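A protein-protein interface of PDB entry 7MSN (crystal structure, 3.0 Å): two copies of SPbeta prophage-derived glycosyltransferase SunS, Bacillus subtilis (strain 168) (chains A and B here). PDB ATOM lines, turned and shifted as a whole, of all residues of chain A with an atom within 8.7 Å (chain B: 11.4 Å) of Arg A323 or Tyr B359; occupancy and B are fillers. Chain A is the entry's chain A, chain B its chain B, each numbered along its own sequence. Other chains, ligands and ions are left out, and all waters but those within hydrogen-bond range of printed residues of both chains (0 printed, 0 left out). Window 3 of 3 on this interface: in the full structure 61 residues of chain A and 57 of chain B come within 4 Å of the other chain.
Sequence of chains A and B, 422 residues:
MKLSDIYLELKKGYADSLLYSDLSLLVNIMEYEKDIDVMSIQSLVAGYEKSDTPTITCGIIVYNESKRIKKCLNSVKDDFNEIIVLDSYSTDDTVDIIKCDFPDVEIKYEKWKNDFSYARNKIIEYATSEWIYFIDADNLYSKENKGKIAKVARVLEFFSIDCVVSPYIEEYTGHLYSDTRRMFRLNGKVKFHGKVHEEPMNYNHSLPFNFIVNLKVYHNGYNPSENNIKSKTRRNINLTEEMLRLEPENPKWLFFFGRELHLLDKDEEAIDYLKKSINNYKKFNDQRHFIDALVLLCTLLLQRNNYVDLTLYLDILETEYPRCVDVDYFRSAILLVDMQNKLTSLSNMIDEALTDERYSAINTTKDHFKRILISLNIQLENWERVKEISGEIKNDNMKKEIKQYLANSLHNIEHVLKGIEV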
ATOM      1  N   HIS A 175       3.646  41.413  -3.321  1.00  0.00           N
ATOM      2  CA  HIS A 175       2.620  40.488  -2.876  1.00  0.00           C
ATOM      3  C   HIS A 175       1.325  41.245  -2.644  1.00  0.00           C
ATOM      4  O   HIS A 175       1.346  42.348  -2.092  1.00  0.00           O
ATOM      5  CB  HIS A 175       3.127  39.834  -1.599  1.00  0.00           C
ATOM      6  CG  HIS A 175       2.143  38.980  -0.871  1.00  0.00           C
ATOM      7  ND1 HIS A 175       1.600  37.840  -1.414  1.00  0.00           N
ATOM      8  CD2 HIS A 175       1.709  39.029   0.408  1.00  0.00           C
ATOM      9  CE1 HIS A 175       0.822  37.254  -0.523  1.00  0.00           C
ATOM     10  NE2 HIS A 175       0.868  37.959   0.591  1.00  0.00           N
ATOM     11  N   ARG A 288      -8.125  31.873   9.546  1.00  0.00           N
ATOM     12  CA  ARG A 288      -7.681  32.747   8.455  1.00  0.00           C
ATOM     13  C   ARG A 288      -6.173  32.720   8.286  1.00  0.00           C
ATOM     14  O   ARG A 288      -5.676  32.529   7.170  1.00  0.00           O
ATOM     15  CB  ARG A 288      -8.158  34.189   8.655  1.00  0.00           C
ATOM     16  CG  ARG A 288      -9.390  34.501   7.852  1.00  0.00           C
ATOM     17  CD  ARG A 288      -9.887  35.884   8.086  1.00  0.00           C
ATOM     18  NE  ARG A 288     -10.286  36.076   9.465  1.00  0.00           N
ATOM     19  CZ  ARG A 288     -10.290  37.259  10.049  1.00  0.00           C
ATOM     20  NH1 ARG A 288      -9.927  38.328   9.367  1.00  0.00           N
ATOM     21  NH2 ARG A 288     -10.645  37.382  11.310  1.00  0.00           N
ATOM     22  N   ILE A 291      -2.791  29.378   7.326  1.00  0.00           N
ATOM     23  CA  ILE A 291      -1.866  29.114   6.229  1.00  0.00           C
ATOM     24  C   ILE A 291      -0.611  29.965   6.379  1.00  0.00           C
ATOM     25  O   ILE A 291       0.511  29.497   6.156  1.00  0.00           O
ATOM     26  CB  ILE A 291      -2.570  29.324   4.872  1.00  0.00           C
ATOM     27  CG1 ILE A 291      -1.702  28.823   3.720  1.00  0.00           C
ATOM     28  CG2 ILE A 291      -2.937  30.773   4.646  1.00  0.00           C
ATOM     29  CD1 ILE A 291      -2.450  28.666   2.438  1.00  0.00           C
ATOM     30  N   ASP A 292      -0.777  31.203   6.824  1.00  0.00           N
ATOM     31  CA  ASP A 292       0.365  32.089   6.983  1.00  0.00           C
ATOM     32  C   ASP A 292       1.311  31.596   8.063  1.00  0.00           C
ATOM     33  O   ASP A 292       2.530  31.793   7.969  1.00  0.00           O
ATOM     34  CB  ASP A 292      -0.140  33.484   7.308  1.00  0.00           C
ATOM     35  CG  ASP A 292      -0.674  34.174   6.101  1.00  0.00           C
ATOM     36  OD1 ASP A 292       0.087  34.278   5.088  1.00  0.00           O
ATOM     37  OD2 ASP A 292      -1.866  34.545   6.161  1.00  0.00           O
ATOM     38  N   VAL A 295       3.386  28.595   6.297  1.00  0.00           N
ATOM     39  CA  VAL A 295       4.377  28.927   5.283  1.00  0.00           C
ATOM     40  C   VAL A 295       5.511  29.734   5.887  1.00  0.00           C
ATOM     41  O   VAL A 295       6.659  29.658   5.420  1.00  0.00           O
ATOM     42  CB  VAL A 295       3.740  29.661   4.094  1.00  0.00           C
ATOM     43  CG1 VAL A 295       2.742  28.733   3.399  1.00  0.00           C
ATOM     44  CG2 VAL A 295       3.128  30.954   4.525  1.00  0.00           C
ATOM     45  N   LEU A 317       0.940  21.416   5.904  1.00  0.00           N
ATOM     46  CA  LEU A 317       0.603  22.394   4.879  1.00  0.00           C
ATOM     47  C   LEU A 317      -0.122  21.737   3.725  1.00  0.00           C
ATOM     48  O   LEU A 317      -1.099  22.284   3.210  1.00  0.00           O
ATOM     49  CB  LEU A 317       1.855  23.105   4.374  1.00  0.00           C
ATOM     50  CG  LEU A 317       1.539  24.069   3.223  1.00  0.00           C
ATOM     51  CD1 LEU A 317       0.677  25.240   3.684  1.00  0.00           C
ATOM     52  CD2 LEU A 317       2.823  24.572   2.571  1.00  0.00           C
ATOM     53  N   GLU A 318       0.319  20.547   3.322  1.00  0.00           N
ATOM     54  CA  GLU A 318      -0.276  19.932   2.145  1.00  0.00           C
ATOM     55  C   GLU A 318      -1.661  19.352   2.434  1.00  0.00           C
ATOM     56  O   GLU A 318      -2.538  19.412   1.571  1.00  0.00           O
ATOM     57  CB  GLU A 318       0.659  18.871   1.590  1.00  0.00           C
ATOM     58  CG  GLU A 318       0.123  18.198   0.350  1.00  0.00           C
ATOM     59  CD  GLU A 318       1.198  17.504  -0.474  1.00  0.00           C
ATOM     60  OE1 GLU A 318       2.257  17.121   0.097  1.00  0.00           O
ATOM     61  OE2 GLU A 318       0.963  17.324  -1.692  1.00  0.00           O
ATOM     62  N   THR A 319      -1.894  18.788   3.626  1.00  0.00           N
ATOM     63  CA  THR A 319      -3.204  18.169   3.860  1.00  0.00           C
ATOM     64  C   THR A 319      -4.300  19.224   4.001  1.00  0.00           C
ATOM     65  O   THR A 319      -5.452  18.980   3.614  1.00  0.00           O
ATOM     66  CB  THR A 319      -3.208  17.288   5.123  1.00  0.00           C
ATOM     67  OG1 THR A 319      -3.014  18.103   6.279  1.00  0.00           O
ATOM     68  CG2 THR A 319      -2.078  16.260   5.096  1.00  0.00           C
ATOM     69  N   GLU A 320      -3.939  20.405   4.532  1.00  0.00           N
ATOM     70  CA  GLU A 320      -4.845  21.483   4.920  1.00  0.00           C
ATOM     71  C   GLU A 320      -5.128  22.465   3.781  1.00  0.00           C
ATOM     72  O   GLU A 320      -6.215  23.064   3.740  1.00  0.00           O
ATOM     73  CB  GLU A 320      -4.235  22.266   6.089  1.00  0.00           C
ATOM     74  CG  GLU A 320      -4.210  21.528   7.436  1.00  0.00           C
ATOM     75  CD  GLU A 320      -5.562  21.419   8.144  1.00  0.00           C
ATOM     76  OE1 GLU A 320      -6.521  22.166   7.797  1.00  0.00           O
ATOM     77  OE2 GLU A 320      -5.662  20.550   9.043  1.00  0.00           O
ATOM     78  N   TYR A 321      -4.163  22.659   2.873  1.00  0.00           N
ATOM     79  CA  TYR A 321      -4.264  23.636   1.789  1.00  0.00           C
ATOM     80  C   TYR A 321      -3.643  23.037   0.541  1.00  0.00           C
ATOM     81  O   TYR A 321      -2.622  23.515   0.040  1.00  0.00           O
ATOM     82  CB  TYR A 321      -3.596  24.961   2.177  1.00  0.00           C
ATOM     83  CG  TYR A 321      -4.229  25.589   3.391  1.00  0.00           C
ATOM     84  CD1 TYR A 321      -3.636  25.503   4.644  1.00  0.00           C
ATOM     85  CD2 TYR A 321      -5.479  26.187   3.298  1.00  0.00           C
ATOM     86  CE1 TYR A 321      -4.241  26.056   5.765  1.00  0.00           C
ATOM     87  CE2 TYR A 321      -6.092  26.730   4.405  1.00  0.00           C
ATOM     88  CZ  TYR A 321      -5.472  26.661   5.632  1.00  0.00           C
ATOM     89  OH  TYR A 321      -6.113  27.193   6.716  1.00  0.00           O
ATOM     90  N   PRO A 322      -4.259  21.987  -0.005  1.00  0.00           N
ATOM     91  CA  PRO A 322      -3.586  21.196  -1.049  1.00  0.00           C
ATOM     92  C   PRO A 322      -3.283  21.969  -2.321  1.00  0.00           C
ATOM     93  O   PRO A 322      -2.287  21.703  -3.012  1.00  0.00           O
ATOM     94  CB  PRO A 322      -4.583  20.061  -1.292  1.00  0.00           C
ATOM     95  CG  PRO A 322      -5.414  20.011  -0.041  1.00  0.00           C
ATOM     96  CD  PRO A 322      -5.557  21.408   0.370  1.00  0.00           C
ATOM     97  N   ARG A 323      -4.094  22.955  -2.629  1.00  0.00           N
ATOM     98  CA  ARG A 323      -3.948  23.744  -3.832  1.00  0.00           C
ATOM     99  C   ARG A 323      -3.054  24.975  -3.632  1.00  0.00           C
ATOM    100  O   ARG A 323      -3.122  25.919  -4.430  1.00  0.00           O
ATOM    101  CB  ARG A 323      -5.336  24.149  -4.307  1.00  0.00           C
ATOM    102  CG  ARG A 323      -5.881  25.215  -3.392  1.00  0.00           C
ATOM    103  CD  ARG A 323      -6.413  24.635  -2.097  1.00  0.00           C
ATOM    104  NE  ARG A 323      -7.122  25.624  -1.333  1.00  0.00           N
ATOM    105  CZ  ARG A 323      -7.509  25.408  -0.101  1.00  0.00           C
ATOM    106  NH1 ARG A 323      -8.160  26.349   0.572  1.00  0.00           N
ATOM    107  NH2 ARG A 323      -7.286  24.218   0.422  1.00  0.00           N
ATOM    108  N   CYS A 324      -2.224  25.000  -2.588  1.00  0.00           N
ATOM    109  CA  CYS A 324      -1.271  26.088  -2.402  1.00  0.00           C
ATOM    110  C   CYS A 324       0.001  25.751  -3.148  1.00  0.00           C
ATOM    111  O   CYS A 324       0.672  24.773  -2.822  1.00  0.00           O
ATOM    112  CB  CYS A 324      -0.955  26.328  -0.932  1.00  0.00           C
ATOM    113  SG  CYS A 324       0.077  27.813  -0.712  1.00  0.00           S
ATOM    114  N   VAL A 325       0.348  26.566  -4.139  1.00  0.00           N
ATOM    115  CA  VAL A 325       1.521  26.242  -4.928  1.00  0.00           C
ATOM    116  C   VAL A 325       2.793  26.269  -4.070  1.00  0.00           C
ATOM    117  O   VAL A 325       3.804  25.646  -4.430  1.00  0.00           O
ATOM    118  CB  VAL A 325       1.592  27.196  -6.140  1.00  0.00           C
ATOM    119  CG1 VAL A 325       1.962  28.605  -5.712  1.00  0.00           C
ATOM    120  CG2 VAL A 325       2.532  26.662  -7.194  1.00  0.00           C
ATOM    121  N   ASP A 326       2.751  26.939  -2.912  1.00  0.00           N
ATOM    122  CA  ASP A 326       3.917  27.010  -2.039  1.00  0.00           C
ATOM    123  C   ASP A 326       4.314  25.652  -1.484  1.00  0.00           C
ATOM    124  O   ASP A 326       5.453  25.500  -1.025  1.00  0.00           O
ATOM    125  CB  ASP A 326       3.657  27.948  -0.873  1.00  0.00           C
ATOM    126  CG  ASP A 326       3.656  29.388  -1.281  1.00  0.00           C
ATOM    127  OD1 ASP A 326       2.791  30.124  -0.769  1.00  0.00           O
ATOM    128  OD2 ASP A 326       4.513  29.787  -2.106  1.00  0.00           O
ATOM    129  N   VAL A 327       3.404  24.668  -1.486  1.00  0.00           N
ATOM    130  CA  VAL A 327       3.820  23.301  -1.173  1.00  0.00           C
ATOM    131  C   VAL A 327       4.953  22.886  -2.102  1.00  0.00           C
ATOM    132  O   VAL A 327       6.034  22.486  -1.656  1.00  0.00           O
ATOM    133  CB  VAL A 327       2.634  22.323  -1.277  1.00  0.00           C
ATOM    134  CG1 VAL A 327       3.149  20.919  -1.302  1.00  0.00           C
ATOM    135  CG2 VAL A 327       1.641  22.507  -0.127  1.00  0.00           C
ATOM    136  N   ASP A 328       4.726  23.036  -3.417  1.00  0.00           N
ATOM    137  CA  ASP A 328       5.685  22.611  -4.429  1.00  0.00           C
ATOM    138  C   ASP A 328       6.993  23.375  -4.314  1.00  0.00           C
ATOM    139  O   ASP A 328       8.073  22.802  -4.495  1.00  0.00           O
ATOM    140  CB  ASP A 328       5.084  22.789  -5.820  1.00  0.00           C
ATOM    141  CG  ASP A 328       3.897  21.856  -6.076  1.00  0.00           C
ATOM    142  OD1 ASP A 328       3.952  20.681  -5.648  1.00  0.00           O
ATOM    143  OD2 ASP A 328       2.903  22.288  -6.704  1.00  0.00           O
ATOM    144  N   GLU B 352       5.523  23.307 -14.723  1.00  0.00           N
ATOM    145  CA  GLU B 352       4.175  22.738 -14.658  1.00  0.00           C
ATOM    146  C   GLU B 352       3.396  23.265 -13.466  1.00  0.00           C
ATOM    147  O   GLU B 352       2.177  23.459 -13.548  1.00  0.00           O
ATOM    148  CB  GLU B 352       4.233  21.209 -14.581  1.00  0.00           C
ATOM    149  CG  GLU B 352       4.688  20.533 -15.855  1.00  0.00           C
ATOM    150  CD  GLU B 352       3.713  20.784 -17.001  1.00  0.00           C
ATOM    151  OE1 GLU B 352       2.518  21.073 -16.731  1.00  0.00           O
ATOM    152  OE2 GLU B 352       4.149  20.714 -18.172  1.00  0.00           O
ATOM    153  N   ALA B 353       4.074  23.459 -12.335  1.00  0.00           N
ATOM    154  CA  ALA B 353       3.387  23.968 -11.157  1.00  0.00           C
ATOM    155  C   ALA B 353       2.943  25.411 -11.361  1.00  0.00           C
ATOM    156  O   ALA B 353       1.801  25.764 -11.035  1.00  0.00           O
ATOM    157  CB  ALA B 353       4.285  23.845  -9.928  1.00  0.00           C
ATOM    158  N   LEU B 354       3.823  26.252 -11.914  1.00  0.00           N
ATOM    159  CA  LEU B 354       3.522  27.673 -12.025  1.00  0.00           C
ATOM    160  C   LEU B 354       2.305  27.940 -12.900  1.00  0.00           C
ATOM    161  O   LEU B 354       1.631  28.961 -12.715  1.00  0.00           O
ATOM    162  CB  LEU B 354       4.741  28.432 -12.562  1.00  0.00           C
ATOM    163  CG  LEU B 354       5.941  28.584 -11.622  1.00  0.00           C
ATOM    164  CD1 LEU B 354       6.879  29.705 -12.076  1.00  0.00           C
ATOM    165  CD2 LEU B 354       5.441  28.835 -10.219  1.00  0.00           C
ATOM    166  N   THR B 355       1.987  27.030 -13.817  1.00  0.00           N
ATOM    167  CA  THR B 355       0.938  27.247 -14.799  1.00  0.00           C
ATOM    168  C   THR B 355      -0.409  26.679 -14.373  1.00  0.00           C
ATOM    169  O   THR B 355      -1.269  26.448 -15.228  1.00  0.00           O
ATOM    170  CB  THR B 355       1.340  26.646 -16.143  1.00  0.00           C
ATOM    171  OG1 THR B 355       0.389  27.059 -17.129  1.00  0.00           O
ATOM    172  CG2 THR B 355       1.360  25.110 -16.064  1.00  0.00           C
ATOM    173  N   ASP B 356      -0.615  26.434 -13.090  1.00  0.00           N
ATOM    174  CA  ASP B 356      -1.955  26.104 -12.644  1.00  0.00           C
ATOM    175  C   ASP B 356      -2.667  27.367 -12.178  1.00  0.00           C
ATOM    176  O   ASP B 356      -2.123  28.475 -12.181  1.00  0.00           O
ATOM    177  CB  ASP B 356      -1.945  25.066 -11.519  1.00  0.00           C
ATOM    178  CG  ASP B 356      -1.415  23.718 -11.961  1.00  0.00           C
ATOM    179  OD1 ASP B 356      -1.513  23.410 -13.170  1.00  0.00           O
ATOM    180  OD2 ASP B 356      -0.927  22.958 -11.093  1.00  0.00           O
ATOM    181  N   GLU B 357      -3.916  27.187 -11.775  1.00  0.00           N
ATOM    182  CA  GLU B 357      -4.604  28.204 -10.997  1.00  0.00           C
ATOM    183  C   GLU B 357      -4.007  28.406  -9.599  1.00  0.00           C
ATOM    184  O   GLU B 357      -4.406  29.354  -8.904  1.00  0.00           O
ATOM    185  CB  GLU B 357      -6.103  27.842 -10.925  1.00  0.00           C
ATOM    186  CG  GLU B 357      -6.452  26.427 -10.367  1.00  0.00           C
ATOM    187  CD  GLU B 357      -6.401  26.258  -8.830  1.00  0.00           C
ATOM    188  OE1 GLU B 357      -6.281  27.258  -8.076  1.00  0.00           O
ATOM    189  OE2 GLU B 357      -6.500  25.089  -8.380  1.00  0.00           O
ATOM    190  N   ARG B 358      -3.046  27.578  -9.179  1.00  0.00           N
ATOM    191  CA  ARG B 358      -2.747  27.476  -7.758  1.00  0.00           C
ATOM    192  C   ARG B 358      -2.040  28.724  -7.233  1.00  0.00           C
ATOM    193  O   ARG B 358      -1.030  29.184  -7.783  1.00  0.00           O
ATOM    194  CB  ARG B 358      -1.956  26.206  -7.475  1.00  0.00           C
ATOM    195  CG  ARG B 358      -2.871  25.013  -7.592  1.00  0.00           C
ATOM    196  CD  ARG B 358      -2.234  23.655  -7.329  1.00  0.00           C
ATOM    197  NE  ARG B 358      -1.042  23.420  -8.134  1.00  0.00           N
ATOM    198  CZ  ARG B 358       0.148  23.117  -7.633  1.00  0.00           C
ATOM    199  NH1 ARG B 358       0.303  22.946  -6.322  1.00  0.00           N
ATOM    200  NH2 ARG B 358       1.172  22.936  -8.452  1.00  0.00           N
ATOM    201  N   TYR B 359      -2.609  29.258  -6.155  1.00  0.00           N
ATOM    202  CA  TYR B 359      -2.244  30.485  -5.472  1.00  0.00           C
ATOM    203  C   TYR B 359      -1.018  30.309  -4.583  1.00  0.00           C
ATOM    204  O   TYR B 359      -0.676  29.199  -4.161  1.00  0.00           O
ATOM    205  CB  TYR B 359      -3.422  30.952  -4.624  1.00  0.00           C
ATOM    206  CG  TYR B 359      -3.739  30.093  -3.388  1.00  0.00           C
ATOM    207  CD1 TYR B 359      -3.184  30.384  -2.152  1.00  0.00           C
ATOM    208  CD2 TYR B 359      -4.626  29.020  -3.460  1.00  0.00           C
ATOM    209  CE1 TYR B 359      -3.475  29.634  -1.050  1.00  0.00           C
ATOM    210  CE2 TYR B 359      -4.927  28.273  -2.355  1.00  0.00           C
ATOM    211  CZ  TYR B 359      -4.349  28.580  -1.145  1.00  0.00           C
ATOM    212  OH  TYR B 359      -4.642  27.841  -0.001  1.00  0.00           O
ATOM    213  N   SER B 360      -0.376  31.435  -4.262  1.00  0.00           N
ATOM    214  CA  SER B 360       0.711  31.487  -3.294  1.00  0.00           C
ATOM    215  C   SER B 360       0.293  32.281  -2.063  1.00  0.00           C
ATOM    216  O   SER B 360      -0.347  33.326  -2.178  1.00  0.00           O
ATOM    217  CB  SER B 360       1.946  32.126  -3.902  1.00  0.00           C
ATOM    218  OG  SER B 360       2.912  32.333  -2.902  1.00  0.00           O
ATOM    219  N   ALA B 361       0.646  31.782  -0.880  1.00  0.00           N
ATOM    220  CA  ALA B 361       0.470  32.556   0.345  1.00  0.00           C
ATOM    221  C   ALA B 361       1.721  33.317   0.731  1.00  0.00           C
ATOM    222  O   ALA B 361       1.639  34.221   1.573  1.00  0.00           O
ATOM    223  CB  ALA B 361       0.073  31.655   1.516  1.00  0.00           C
ATOM    224  N   ILE B 362       2.863  32.958   0.141  1.00  0.00           N
ATOM    225  CA  ILE B 362       4.133  33.604   0.454  1.00  0.00           C
ATOM    226  C   ILE B 362       4.299  34.883  -0.361  1.00  0.00           C
ATOM    227  O   ILE B 362       4.422  35.988   0.177  1.00  0.00           O
ATOM    228  CB  ILE B 362       5.297  32.624   0.201  1.00  0.00           C
ATOM    229  CG1 ILE B 362       5.392  31.585   1.312  1.00  0.00           C
ATOM    230  CG2 ILE B 362       6.614  33.357   0.061  1.00  0.00           C
ATOM    231  CD1 ILE B 362       6.320  30.444   0.994  1.00  0.00           C
ATOM    232  N   ASN B 363       4.334  34.743  -1.680  1.00  0.00           N
ATOM    233  CA  ASN B 363       4.425  35.868  -2.603  1.00  0.00           C
ATOM    234  C   ASN B 363       3.455  35.563  -3.732  1.00  0.00           C
ATOM    235  O   ASN B 363       3.674  34.641  -4.523  1.00  0.00           O
ATOM    236  CB  ASN B 363       5.851  36.076  -3.126  1.00  0.00           C
ATOM    237  CG  ASN B 363       6.035  37.434  -3.781  1.00  0.00           C
ATOM    238  OD1 ASN B 363       5.052  38.081  -4.134  1.00  0.00           O
ATOM    239  ND2 ASN B 363       7.284  37.892  -3.901  1.00  0.00           N
ATOM    240  N   THR B 364       2.372  36.326  -3.790  1.00  0.00           N
ATOM    241  CA  THR B 364       1.308  36.035  -4.730  1.00  0.00           C
ATOM    242  C   THR B 364       1.790  36.104  -6.177  1.00  0.00           C
ATOM    243  O   THR B 364       1.129  35.562  -7.073  1.00  0.00           O
ATOM    244  CB  THR B 364       0.164  37.009  -4.477  1.00  0.00           C
ATOM    245  OG1 THR B 364      -0.965  36.573  -5.220  1.00  0.00           O
ATOM    246  CG2 THR B 364       0.520  38.365  -4.976  1.00  0.00           C
ATOM    247  N   THR B 365       2.939  36.747  -6.415  1.00  0.00           N
ATOM    248  CA  THR B 365       3.566  36.903  -7.720  1.00  0.00           C
ATOM    249  C   THR B 365       4.428  35.698  -8.101  1.00  0.00           C
ATOM    250  O   THR B 365       5.166  35.758  -9.098  1.00  0.00           O
ATOM    251  CB  THR B 365       4.389  38.209  -7.742  1.00  0.00           C
ATOM    252  OG1 THR B 365       5.502  38.122  -6.860  1.00  0.00           O
ATOM    253  CG2 THR B 365       3.556  39.367  -7.273  1.00  0.00           C
ATOM    254  N   LYS B 366       4.329  34.612  -7.325  1.00  0.00           N
ATOM    255  CA  LYS B 366       5.074  33.374  -7.519  1.00  0.00           C
ATOM    256  C   LYS B 366       6.526  33.698  -7.854  1.00  0.00           C
ATOM    257  O   LYS B 366       7.197  32.971  -8.588  1.00  0.00           O
ATOM    258  CB  LYS B 366       4.383  32.518  -8.578  1.00  0.00           C
ATOM    259  CG  LYS B 366       2.883  32.612  -8.466  1.00  0.00           C
ATOM    260  CD  LYS B 366       2.215  31.366  -8.923  1.00  0.00           C
ATOM    261  CE  LYS B 366       0.793  31.627  -9.339  1.00  0.00           C
ATOM    262  NZ  LYS B 366       0.258  30.377  -9.923  1.00  0.00           N
ATOM    263  N   ASP B 367       7.021  34.782  -7.267  1.00  0.00           N
ATOM    264  CA  ASP B 367       8.283  35.401  -7.631  1.00  0.00           C
ATOM    265  C   ASP B 367       9.443  34.788  -6.854  1.00  0.00           C
ATOM    266  O   ASP B 367      10.597  34.977  -7.240  1.00  0.00           O
ATOM    267  CB  ASP B 367       8.134  36.930  -7.404  1.00  0.00           C
ATOM    268  CG  ASP B 367       9.265  37.787  -7.992  1.00  0.00           C
ATOM    269  OD1 ASP B 367       9.283  37.933  -9.229  1.00  0.00           O
ATOM    270  OD2 ASP B 367      10.020  38.435  -7.233  1.00  0.00           O
ATOM    271  N   HIS B 368       9.149  34.021  -5.792  1.00  0.00           N
ATOM    272  CA  HIS B 368      10.156  33.250  -5.063  1.00  0.00           C
ATOM    273  C   HIS B 368      10.475  31.951  -5.789  1.00  0.00           C
ATOM    274  O   HIS B 368      11.578  31.412  -5.648  1.00  0.00           O
ATOM    275  CB  HIS B 368       9.678  32.926  -3.636  1.00  0.00           C
ATOM    276  CG  HIS B 368       8.301  32.319  -3.555  1.00  0.00           C
ATOM    277  ND1 HIS B 368       7.179  32.903  -4.102  1.00  0.00           N
ATOM    278  CD2 HIS B 368       7.862  31.197  -2.931  1.00  0.00           C
ATOM    279  CE1 HIS B 368       6.120  32.153  -3.856  1.00  0.00           C
ATOM    280  NE2 HIS B 368       6.505  31.117  -3.135  1.00  0.00           N
ATOM    281  N   PHE B 369       9.497  31.425  -6.535  1.00  0.00           N
ATOM    282  CA  PHE B 369       9.750  30.335  -7.464  1.00  0.00           C
ATOM    283  C   PHE B 369      10.795  30.736  -8.473  1.00  0.00           C
ATOM    284  O   PHE B 369      11.508  29.887  -9.004  1.00  0.00           O
ATOM    285  CB  PHE B 369       8.483  29.975  -8.224  1.00  0.00           C
ATOM    286  CG  PHE B 369       7.602  29.002  -7.523  1.00  0.00           C
ATOM    287  CD1 PHE B 369       7.646  27.660  -7.837  1.00  0.00           C
ATOM    288  CD2 PHE B 369       6.689  29.445  -6.577  1.00  0.00           C
ATOM    289  CE1 PHE B 369       6.814  26.778  -7.218  1.00  0.00           C
ATOM    290  CE2 PHE B 369       5.852  28.568  -5.944  1.00  0.00           C
ATOM    291  CZ  PHE B 369       5.915  27.229  -6.256  1.00  0.00           C
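The side-chain sulfur (SG) of Cys A324 is in hydrogen-bond range of the side-chain carboxylate (OD1) of Asp A326, at 3.6 Å.
NE of Arg B358 is in salt-bridge range of OD2 of Asp B356, at 3.0 Å.
NZ of Lys B366 sits at hydrogen-bond distance from O of Arg B358 (2.8 Å).
The side-chain hydroxyl of Ser B360 is in hydrogen-bond range of the backbone NH of Ile B362 (3.1 Å).
The side-chain hydroxyl (OG) of Ser B360 sits at hydrogen-bond distance from the backbone carbonyl oxygen (O) of Asn B363 (2.9 Å).
OG1 of Thr B365 sits at hydrogen-bond distance from OD1 of Asn B363 (2.8 Å).
Among the printed residues, pairs that only touch across the chains: His A175 with Ala B361 (3.8 Å), His A175 with Ile B362 (3.7 Å), His A175 with Asn B363 (3.6 Å), Ile A291 with Tyr B359 (3.4 Å), Asp A292 with Ala B361 (3.8 Å), Val A295 with Ile B362 (3.8 Å), Tyr A321 with Tyr B359 (3.8 Å), Arg A323 with Arg B358 (3.3 Å), Arg A323 with Tyr B359 (3.4 Å), Cys A324 with Arg B358 (3.97 Å), Val A325 with Arg B358 (3.7 Å), Val A325 with Ser B360 (3.9 Å), Val A325 with Phe B369 (3.2 Å) and Asp A328 with Ala B353 (3.8 Å).
Printed residues of chain A that touch a printed residue of chain B: His A175, Ile A291, Asp A292, Val A295, Tyr A321, Arg A323, Cys A324, Val A325, Asp A326 and Asp A328.
Hydrophobic or aromatic side chains of chain A within 4 Å of the printed part of chain B: His A175, Ile A291, Val A295, Tyr A321 and Val A325.
Along chain A the printed residues that touch a printed residue of chain B span positions 175 to 328.
Among the printed residues, 22 pairs touch across the chains.
A ring nitrogen (ND1) of His A175 is in hydrogen-bond range of the backbone NH (N) of Thr B364, 2.9 Å away.
O of Tyr B359 lies close to SG of Cys A324.
The backbone NH of Val A325 sits at hydrogen-bond distance from the backbone carbonyl oxygen of Tyr B359.
The side-chain carboxylate of Asp A326 sits at hydrogen-bond distance from the side-chain hydroxyl of Ser B360 (3.1 Å).
OD1 of Asp A326 sits at hydrogen-bond distance from N of Ala B361 (2.7 Å).
OD1 of Asp A326 lies within hydrogen-bond range of N of Ile B362, at 3.0 Å.
OD2 of Asp A326 sits at hydrogen-bond distance from NE2 of His B368 (2.6 Å).
The guanidinium group (NH2) of Arg B358 is in salt-bridge range of the side-chain carboxylate (OD2) of Asp A328 (2.5 Å).
No position is printed for both chains.
Of the 22 pairs that touch across the chains among the printed residues, none has its exchanged pair printed and touching as well.
Tyr A321 touches one residue of chain B.
No residue of chain B comes within 4 Å of Pro A322.
Arg A323 touches two residues of chain B.
Of the printed residues of chain B, Asp A326 touches Ser B360 (3.1 Å), Ala B361 (2.7 Å), Ile B362 (3.0 Å) and His B368 (2.6 Å).
Of the printed residues of chain B, Asp A328 touches Ala B353 (3.8 Å) and Arg B358 (2.5 Å).
Of chain A, only Ile A291, Tyr A321, Arg A323, Cys A324 and Val A325 come within 4 Å of Tyr B359.
Of the printed residues of chain A, Ser B360 touches Val A325 (3.9 Å) and Asp A326 (3.1 Å).
The nearest residue of chain B that does not touch Arg A323 is Glu B357 (4.3 Å).
The nearest printed residue of chain B that does not touch Cys A324 is Ala B361 (4.01 Å).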
